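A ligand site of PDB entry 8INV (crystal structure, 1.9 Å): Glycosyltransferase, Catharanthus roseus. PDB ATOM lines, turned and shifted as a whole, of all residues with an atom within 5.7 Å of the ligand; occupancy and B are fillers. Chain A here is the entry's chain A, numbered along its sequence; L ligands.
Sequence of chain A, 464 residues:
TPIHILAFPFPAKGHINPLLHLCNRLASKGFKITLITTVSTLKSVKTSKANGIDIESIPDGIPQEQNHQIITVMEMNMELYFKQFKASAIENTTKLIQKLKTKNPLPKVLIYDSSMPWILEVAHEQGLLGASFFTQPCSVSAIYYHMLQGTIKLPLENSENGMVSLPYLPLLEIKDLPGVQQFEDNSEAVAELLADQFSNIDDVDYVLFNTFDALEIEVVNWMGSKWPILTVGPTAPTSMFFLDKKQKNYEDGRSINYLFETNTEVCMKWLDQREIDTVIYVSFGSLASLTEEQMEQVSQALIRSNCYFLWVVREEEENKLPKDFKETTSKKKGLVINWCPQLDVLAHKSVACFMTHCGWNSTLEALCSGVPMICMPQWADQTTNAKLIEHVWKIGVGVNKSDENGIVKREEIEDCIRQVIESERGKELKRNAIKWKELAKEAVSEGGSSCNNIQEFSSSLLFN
CZ of Phe 10 touches O2 of the ligand, 3.6 Å away. His 15 touches the ligand. Ile 71 touches the ligand. Met 78 touches the ligand (CE to O2, 3.5 Å). Ser 115 touches the ligand (CB to O3, 3.0 Å). Gln 136 touches the ligand. CZ of Phe 183 touches C4 of the ligand (3.6 Å). CD2 of Leu 194 touches O4 of the ligand, 3.4 Å away. Leu 287 touches the ligand (CD1 to C17, 3.5 Å). Trp 379 touches the ligand (CZ2 to C9, 3.5 Å). Hydrophobic or aromatic side chains that line the ligand: Phe 10, His 15, Ile 71, Met 78, Phe 183, Leu 194, Leu 287 and Trp 379. 12 residues have an atom within 4 Å of the ligand: Phe 10, His 15, Ile 71, Glu 75, Met 78, Ser 115, Gln 136, Phe 183, Leu 194, Gln 197, Leu 287 and Trp 379.
The backbone carbonyl oxygen (O) of Glu 75 lies within hydrogen-bond range of the side-chain amide nitrogen (ND2) of Asn 186 (2.9 Å). OD2 of Asp 381 sits close to OE1 of Gln 136. The backbone NH (N) of Met 78 lies within hydrogen-bond range of the side-chain amide oxygen (OD1) of Asn 186. OG of Ser 114 is in hydrogen-bond range of OE1 of Gln 197. The side-chain amide nitrogen of Gln 197 lies close to the backbone carbonyl oxygen of Leu 194 (3.4 Å). The side-chain hydroxyl (OG) of Ser 115 is in hydrogen-bond range of the side-chain carboxylate (OD2) of Asp 113, 2.7 Å away. ND1 of His 15 is in hydrogen-bond range of OD1 of Asp 113, 2.8 Å away.
OE2 of Glu 75 is in hydrogen-bond range of O1 of the ligand (3.0 Å). The side-chain amide nitrogen (NE2) of Gln 197 sits at hydrogen-bond distance from an oxygen (O3) of the ligand, at 3.1 Å.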
ATOM      1  N   PHE A  10       5.041 -13.323 -11.431  1.00  0.00           N
ATOM      2  CA  PHE A  10       5.993 -13.743 -12.454  1.00  0.00           C
ATOM      3  C   PHE A  10       5.401 -14.953 -13.188  1.00  0.00           C
ATOM      4  O   PHE A  10       4.704 -15.758 -12.567  1.00  0.00           O
ATOM      5  CB  PHE A  10       7.343 -14.093 -11.803  1.00  0.00           C
ATOM      6  CG  PHE A  10       8.428 -14.480 -12.775  1.00  0.00           C
ATOM      7  CD1 PHE A  10       9.193 -13.514 -13.429  1.00  0.00           C
ATOM      8  CD2 PHE A  10       8.652 -15.821 -13.067  1.00  0.00           C
ATOM      9  CE1 PHE A  10      10.186 -13.886 -14.338  1.00  0.00           C
ATOM     10  CE2 PHE A  10       9.650 -16.201 -13.965  1.00  0.00           C
ATOM     11  CZ  PHE A  10      10.413 -15.239 -14.602  1.00  0.00           C
ATOM     12  N   ALA A  12       5.385 -18.108 -13.911  1.00  0.00           N
ATOM     13  CA  ALA A  12       5.775 -19.483 -13.623  1.00  0.00           C
ATOM     14  C   ALA A  12       4.883 -19.977 -12.491  1.00  0.00           C
ATOM     15  O   ALA A  12       4.439 -19.179 -11.655  1.00  0.00           O
ATOM     16  CB  ALA A  12       7.257 -19.582 -13.231  1.00  0.00           C
ATOM     17  N   HIS A  15       5.163 -19.000  -8.805  1.00  0.00           N
ATOM     18  CA  HIS A  15       4.865 -17.607  -8.515  1.00  0.00           C
ATOM     19  C   HIS A  15       3.389 -17.292  -8.670  1.00  0.00           C
ATOM     20  O   HIS A  15       2.810 -16.606  -7.809  1.00  0.00           O
ATOM     21  CB  HIS A  15       5.727 -16.710  -9.439  1.00  0.00           C
ATOM     22  CG  HIS A  15       7.193 -16.938  -9.257  1.00  0.00           C
ATOM     23  ND1 HIS A  15       7.998 -16.074  -8.542  1.00  0.00           N
ATOM     24  CD2 HIS A  15       7.995 -17.984  -9.615  1.00  0.00           C
ATOM     25  CE1 HIS A  15       9.236 -16.550  -8.504  1.00  0.00           C
ATOM     26  NE2 HIS A  15       9.254 -17.703  -9.150  1.00  0.00           N
ATOM     27  N   ILE A  71       8.847 -19.338 -20.234  1.00  0.00           N
ATOM     28  CA  ILE A  71      10.015 -19.738 -19.465  1.00  0.00           C
ATOM     29  C   ILE A  71      11.042 -20.469 -20.342  1.00  0.00           C
ATOM     30  O   ILE A  71      12.256 -20.313 -20.144  1.00  0.00           O
ATOM     31  CB  ILE A  71       9.568 -20.600 -18.264  1.00  0.00           C
ATOM     32  CG1 ILE A  71       8.780 -19.748 -17.263  1.00  0.00           C
ATOM     33  CG2 ILE A  71      10.733 -21.217 -17.587  1.00  0.00           C
ATOM     34  CD1 ILE A  71       9.521 -18.496 -16.859  1.00  0.00           C
ATOM     35  N   MET A  74      13.022 -17.870 -22.154  1.00  0.00           N
ATOM     36  CA  MET A  74      13.900 -17.077 -21.254  1.00  0.00           C
ATOM     37  C   MET A  74      15.191 -17.851 -20.986  1.00  0.00           C
ATOM     38  O   MET A  74      16.238 -17.224 -20.882  1.00  0.00           O
ATOM     39  CB  MET A  74      13.210 -16.761 -19.920  1.00  0.00           C
ATOM     40  CG  MET A  74      12.876 -15.305 -19.764  1.00  0.00           C
ATOM     41  SD  MET A  74      12.246 -14.955 -18.112  1.00  0.00           S
ATOM     42  CE  MET A  74      10.592 -14.404 -18.508  1.00  0.00           C
ATOM     43  N   GLU A  75      15.087 -19.171 -20.903  1.00  0.00           N
ATOM     44  CA  GLU A  75      16.283 -20.005 -20.657  1.00  0.00           C
ATOM     45  C   GLU A  75      17.314 -19.851 -21.785  1.00  0.00           C
ATOM     46  O   GLU A  75      18.509 -19.939 -21.497  1.00  0.00           O
ATOM     47  CB  GLU A  75      15.853 -21.466 -20.524  1.00  0.00           C
ATOM     48  CG  GLU A  75      16.834 -22.304 -19.725  1.00  0.00           C
ATOM     49  CD  GLU A  75      16.577 -23.791 -19.804  1.00  0.00           C
ATOM     50  OE1 GLU A  75      15.887 -24.226 -20.741  1.00  0.00           O
ATOM     51  OE2 GLU A  75      17.079 -24.523 -18.924  1.00  0.00           O
ATOM     52  N   MET A  78      19.004 -15.606 -20.636  1.00  0.00           N
ATOM     53  CA  MET A  78      18.202 -14.989 -19.577  1.00  0.00           C
ATOM     54  C   MET A  78      18.523 -13.507 -19.431  1.00  0.00           C
ATOM     55  O   MET A  78      17.631 -12.697 -19.165  1.00  0.00           O
ATOM     56  CB  MET A  78      18.389 -15.736 -18.270  1.00  0.00           C
ATOM     57  CG  MET A  78      17.585 -15.134 -17.137  1.00  0.00           C
ATOM     58  SD  MET A  78      15.949 -15.932 -17.102  1.00  0.00           S
ATOM     59  CE  MET A  78      15.333 -15.361 -15.518  1.00  0.00           C
ATOM     60  N   ASP A 113       4.852  -9.693  -8.121  1.00  0.00           N
ATOM     61  CA  ASP A 113       5.935 -10.585  -7.696  1.00  0.00           C
ATOM     62  C   ASP A 113       7.205  -9.802  -7.352  1.00  0.00           C
ATOM     63  O   ASP A 113       7.644  -8.954  -8.124  1.00  0.00           O
ATOM     64  CB  ASP A 113       6.256 -11.581  -8.794  1.00  0.00           C
ATOM     65  CG  ASP A 113       7.030 -12.774  -8.279  1.00  0.00           C
ATOM     66  OD1 ASP A 113       6.417 -13.824  -8.089  1.00  0.00           O
ATOM     67  OD2 ASP A 113       8.249 -12.627  -8.016  1.00  0.00           O
ATOM     68  N   SER A 114       7.813 -10.139  -6.205  1.00  0.00           N
ATOM     69  CA  SER A 114       8.995  -9.404  -5.759  1.00  0.00           C
ATOM     70  C   SER A 114      10.147  -9.478  -6.761  1.00  0.00           C
ATOM     71  O   SER A 114      11.025  -8.594  -6.722  1.00  0.00           O
ATOM     72  CB  SER A 114       9.475  -9.919  -4.387  1.00  0.00           C
ATOM     73  OG  SER A 114       9.973 -11.255  -4.447  1.00  0.00           O
ATOM     74  N   SER A 115      10.148 -10.460  -7.677  1.00  0.00           N
ATOM     75  CA  SER A 115      11.180 -10.558  -8.702  1.00  0.00           C
ATOM     76  C   SER A 115      11.038  -9.515  -9.799  1.00  0.00           C
ATOM     77  O   SER A 115      11.924  -9.451 -10.670  1.00  0.00           O
ATOM     78  CB  SER A 115      11.172 -11.930  -9.366  1.00  0.00           C
ATOM     79  OG  SER A 115       9.943 -12.154 -10.047  1.00  0.00           O
ATOM     80  N   GLN A 136       9.401 -16.586  -1.545  1.00  0.00           N
ATOM     81  CA  GLN A 136      10.440 -17.324  -0.863  1.00  0.00           C
ATOM     82  C   GLN A 136      10.461 -16.898   0.592  1.00  0.00           C
ATOM     83  O   GLN A 136      10.063 -15.779   0.917  1.00  0.00           O
ATOM     84  CB  GLN A 136      11.812 -17.064  -1.519  1.00  0.00           C
ATOM     85  CG  GLN A 136      11.870 -17.549  -2.961  1.00  0.00           C
ATOM     86  CD  GLN A 136      13.269 -17.478  -3.565  1.00  0.00           C
ATOM     87  OE1 GLN A 136      14.254 -17.835  -2.918  1.00  0.00           O
ATOM     88  NE2 GLN A 136      13.354 -17.052  -4.827  1.00  0.00           N
ATOM     89  N   PHE A 183      23.011 -22.858 -13.686  1.00  0.00           N
ATOM     90  CA  PHE A 183      22.427 -22.224 -14.861  1.00  0.00           C
ATOM     91  C   PHE A 183      23.453 -21.898 -15.934  1.00  0.00           C
ATOM     92  O   PHE A 183      23.068 -21.476 -17.028  1.00  0.00           O
ATOM     93  CB  PHE A 183      21.700 -20.954 -14.423  1.00  0.00           C
ATOM     94  CG  PHE A 183      20.649 -21.199 -13.376  1.00  0.00           C
ATOM     95  CD1 PHE A 183      19.793 -22.302 -13.474  1.00  0.00           C
ATOM     96  CD2 PHE A 183      20.566 -20.391 -12.263  1.00  0.00           C
ATOM     97  CE1 PHE A 183      18.836 -22.542 -12.496  1.00  0.00           C
ATOM     98  CE2 PHE A 183      19.608 -20.627 -11.272  1.00  0.00           C
ATOM     99  CZ  PHE A 183      18.751 -21.694 -11.392  1.00  0.00           C
ATOM    100  N   ASN A 186      23.587 -18.575 -17.828  1.00  0.00           N
ATOM    101  CA  ASN A 186      22.584 -17.692 -17.228  1.00  0.00           C
ATOM    102  C   ASN A 186      22.890 -17.356 -15.768  1.00  0.00           C
ATOM    103  O   ASN A 186      22.072 -16.668 -15.132  1.00  0.00           O
ATOM    104  CB  ASN A 186      21.184 -18.331 -17.318  1.00  0.00           C
ATOM    105  CG  ASN A 186      20.669 -18.409 -18.740  1.00  0.00           C
ATOM    106  OD1 ASN A 186      20.925 -17.523 -19.564  1.00  0.00           O
ATOM    107  ND2 ASN A 186      19.891 -19.453 -19.029  1.00  0.00           N
ATOM    108  N   VAL A 190      20.882 -14.626 -13.469  1.00  0.00           N
ATOM    109  CA  VAL A 190      19.957 -15.078 -12.440  1.00  0.00           C
ATOM    110  C   VAL A 190      20.317 -14.451 -11.101  1.00  0.00           C
ATOM    111  O   VAL A 190      19.451 -13.993 -10.351  1.00  0.00           O
ATOM    112  CB  VAL A 190      19.913 -16.614 -12.368  1.00  0.00           C
ATOM    113  CG1 VAL A 190      19.178 -17.052 -11.116  1.00  0.00           C
ATOM    114  CG2 VAL A 190      19.232 -17.181 -13.604  1.00  0.00           C
ATOM    115  N   LEU A 193      19.050 -10.875 -10.755  1.00  0.00           N
ATOM    116  CA  LEU A 193      17.609 -10.716 -10.590  1.00  0.00           C
ATOM    117  C   LEU A 193      17.163 -11.056  -9.169  1.00  0.00           C
ATOM    118  O   LEU A 193      16.224 -10.438  -8.653  1.00  0.00           O
ATOM    119  CB  LEU A 193      16.858 -11.542 -11.619  1.00  0.00           C
ATOM    120  CG  LEU A 193      17.464 -11.346 -12.994  1.00  0.00           C
ATOM    121  CD1 LEU A 193      16.807 -12.252 -14.031  1.00  0.00           C
ATOM    122  CD2 LEU A 193      17.488  -9.855 -13.429  1.00  0.00           C
ATOM    123  N   LEU A 194      17.815 -12.028  -8.536  1.00  0.00           N
ATOM    124  CA  LEU A 194      17.497 -12.331  -7.142  1.00  0.00           C
ATOM    125  C   LEU A 194      17.865 -11.168  -6.242  1.00  0.00           C
ATOM    126  O   LEU A 194      17.057 -10.738  -5.400  1.00  0.00           O
ATOM    127  CB  LEU A 194      18.206 -13.616  -6.696  1.00  0.00           C
ATOM    128  CG  LEU A 194      17.851 -14.850  -7.523  1.00  0.00           C
ATOM    129  CD1 LEU A 194      18.759 -16.040  -7.181  1.00  0.00           C
ATOM    130  CD2 LEU A 194      16.395 -15.208  -7.337  1.00  0.00           C
ATOM    131  N   GLN A 197      15.607  -7.970  -6.029  1.00  0.00           N
ATOM    132  CA  GLN A 197      14.342  -7.952  -5.280  1.00  0.00           C
ATOM    133  C   GLN A 197      14.354  -6.898  -4.163  1.00  0.00           C
ATOM    134  O   GLN A 197      13.286  -6.465  -3.730  1.00  0.00           O
ATOM    135  CB  GLN A 197      14.084  -9.344  -4.720  1.00  0.00           C
ATOM    136  CG  GLN A 197      13.516 -10.298  -5.769  1.00  0.00           C
ATOM    137  CD  GLN A 197      13.298 -11.716  -5.264  1.00  0.00           C
ATOM    138  OE1 GLN A 197      12.352 -11.984  -4.532  1.00  0.00           O
ATOM    139  NE2 GLN A 197      14.200 -12.615  -5.624  1.00  0.00           N
ATOM    140  N   LEU A 287       9.316 -26.646 -13.017  1.00  0.00           N
ATOM    141  CA  LEU A 287      10.400 -26.239 -13.904  1.00  0.00           C
ATOM    142  C   LEU A 287      11.568 -27.204 -13.967  1.00  0.00           C
ATOM    143  O   LEU A 287      12.108 -27.442 -15.054  1.00  0.00           O
ATOM    144  CB  LEU A 287      10.931 -24.861 -13.497  1.00  0.00           C
ATOM    145  CG  LEU A 287       9.926 -23.717 -13.473  1.00  0.00           C
ATOM    146  CD1 LEU A 287      10.518 -22.520 -12.749  1.00  0.00           C
ATOM    147  CD2 LEU A 287       9.493 -23.334 -14.867  1.00  0.00           C
ATOM    148  N   ALA A 288      12.000 -27.756 -12.828  1.00  0.00           N
ATOM    149  CA  ALA A 288      13.187 -28.590 -12.818  1.00  0.00           C
ATOM    150  C   ALA A 288      12.998 -29.817 -13.710  1.00  0.00           C
ATOM    151  O   ALA A 288      11.904 -30.385 -13.787  1.00  0.00           O
ATOM    152  CB  ALA A 288      13.540 -29.012 -11.386  1.00  0.00           C
ATOM    153  N   TRP A 379      18.330 -26.503  -7.834  1.00  0.00           N
ATOM    154  CA  TRP A 379      19.029 -25.236  -8.046  1.00  0.00           C
ATOM    155  C   TRP A 379      18.283 -24.097  -7.355  1.00  0.00           C
ATOM    156  O   TRP A 379      17.253 -24.297  -6.702  1.00  0.00           O
ATOM    157  CB  TRP A 379      19.196 -24.933  -9.551  1.00  0.00           C
ATOM    158  CG  TRP A 379      18.061 -25.393 -10.430  1.00  0.00           C
ATOM    159  CD1 TRP A 379      18.053 -26.471 -11.289  1.00  0.00           C
ATOM    160  CD2 TRP A 379      16.763 -24.792 -10.528  1.00  0.00           C
ATOM    161  NE1 TRP A 379      16.826 -26.551 -11.926  1.00  0.00           N
ATOM    162  CE2 TRP A 379      16.021 -25.551 -11.460  1.00  0.00           C
ATOM    163  CE3 TRP A 379      16.156 -23.697  -9.908  1.00  0.00           C
ATOM    164  CZ2 TRP A 379      14.705 -25.223 -11.812  1.00  0.00           C
ATOM    165  CZ3 TRP A 379      14.844 -23.386 -10.245  1.00  0.00           C
ATOM    166  CH2 TRP A 379      14.132 -24.152 -11.187  1.00  0.00           C
ATOM    167  N   ALA A 380      18.827 -22.895  -7.509  1.00  0.00           N
ATOM    168  CA  ALA A 380      18.326 -21.691  -6.846  1.00  0.00           C
ATOM    169  C   ALA A 380      18.131 -21.919  -5.349  1.00  0.00           C
ATOM    170  O   ALA A 380      18.977 -22.542  -4.689  1.00  0.00           O
ATOM    171  CB  ALA A 380      17.024 -21.196  -7.495  1.00  0.00           C
ATOM    172  N   ASP A 381      17.015 -21.419  -4.810  1.00  0.00           N
ATOM    173  CA  ASP A 381      16.766 -21.469  -3.377  1.00  0.00           C
ATOM    174  C   ASP A 381      16.505 -22.883  -2.877  1.00  0.00           C
ATOM    175  O   ASP A 381      16.439 -23.081  -1.662  1.00  0.00           O
ATOM    176  CB  ASP A 381      15.581 -20.588  -2.995  1.00  0.00           C
ATOM    177  CG  ASP A 381      14.317 -20.932  -3.778  1.00  0.00           C
ATOM    178  OD1 ASP A 381      14.392 -21.054  -5.015  1.00  0.00           O
ATOM    179  OD2 ASP A 381      13.256 -21.103  -3.146  1.00  0.00           O
HETATM  180  C1  LIG L   1      15.120 -17.762 -11.704  1.00  0.00           C
HETATM  181  C2  LIG L   1      14.058 -18.838 -11.981  1.00  0.00           C
HETATM  182  C3  LIG L   1      14.653 -20.229 -11.746  1.00  0.00           C
HETATM  183  C4  LIG L   1      15.628 -20.632 -12.834  1.00  0.00           C
HETATM  184  C5  LIG L   1      14.949 -20.650 -14.210  1.00  0.00           C
HETATM  185  C6  LIG L   1      15.824 -21.263 -15.348  1.00  0.00           C
HETATM  186  C7  LIG L   1      17.133 -20.474 -15.526  1.00  0.00           C
HETATM  187  C8  LIG L   1      16.169 -22.741 -15.063  1.00  0.00           C
HETATM  188  C9  LIG L   1      14.933 -23.624 -14.910  1.00  0.00           C
HETATM  189  C10 LIG L   1      14.013 -23.555 -16.110  1.00  0.00           C
HETATM  190  O1  LIG L   1      14.577 -24.257 -17.225  1.00  0.00           O
HETATM  191  C11 LIG L   1      13.727 -22.115 -16.505  1.00  0.00           C
HETATM  192  C12 LIG L   1      14.967 -21.234 -16.633  1.00  0.00           C
HETATM  193  C13 LIG L   1      14.600 -19.807 -17.007  1.00  0.00           C
HETATM  194  C14 LIG L   1      13.752 -19.166 -15.900  1.00  0.00           C
HETATM  195  C15 LIG L   1      14.432 -19.227 -14.533  1.00  0.00           C
HETATM  196  C16 LIG L   1      13.485 -18.724 -13.427  1.00  0.00           C
HETATM  197  O2  LIG L   1      13.158 -17.338 -13.692  1.00  0.00           O
HETATM  198  C17 LIG L   1      12.146 -19.439 -13.294  1.00  0.00           C
HETATM  199  C18 LIG L   1      11.584 -18.861 -11.989  1.00  0.00           C
HETATM  200  C19 LIG L   1      12.802 -18.628 -11.084  1.00  0.00           C
HETATM  201  C20 LIG L   1      12.776 -17.332 -10.319  1.00  0.00           C
HETATM  202  C21 LIG L   1      12.279 -16.166 -10.893  1.00  0.00           C
HETATM  203  C22 LIG L   1      12.268 -14.984 -10.166  1.00  0.00           C
HETATM  204  C23 LIG L   1      12.771 -14.971  -8.811  1.00  0.00           C
HETATM  205  O3  LIG L   1      12.822 -14.027  -8.066  1.00  0.00           O
HETATM  206  O4  LIG L   1      13.246 -16.131  -8.287  1.00  0.00           O
HETATM  207  C24 LIG L   1      13.256 -17.299  -9.004  1.00  0.00           C
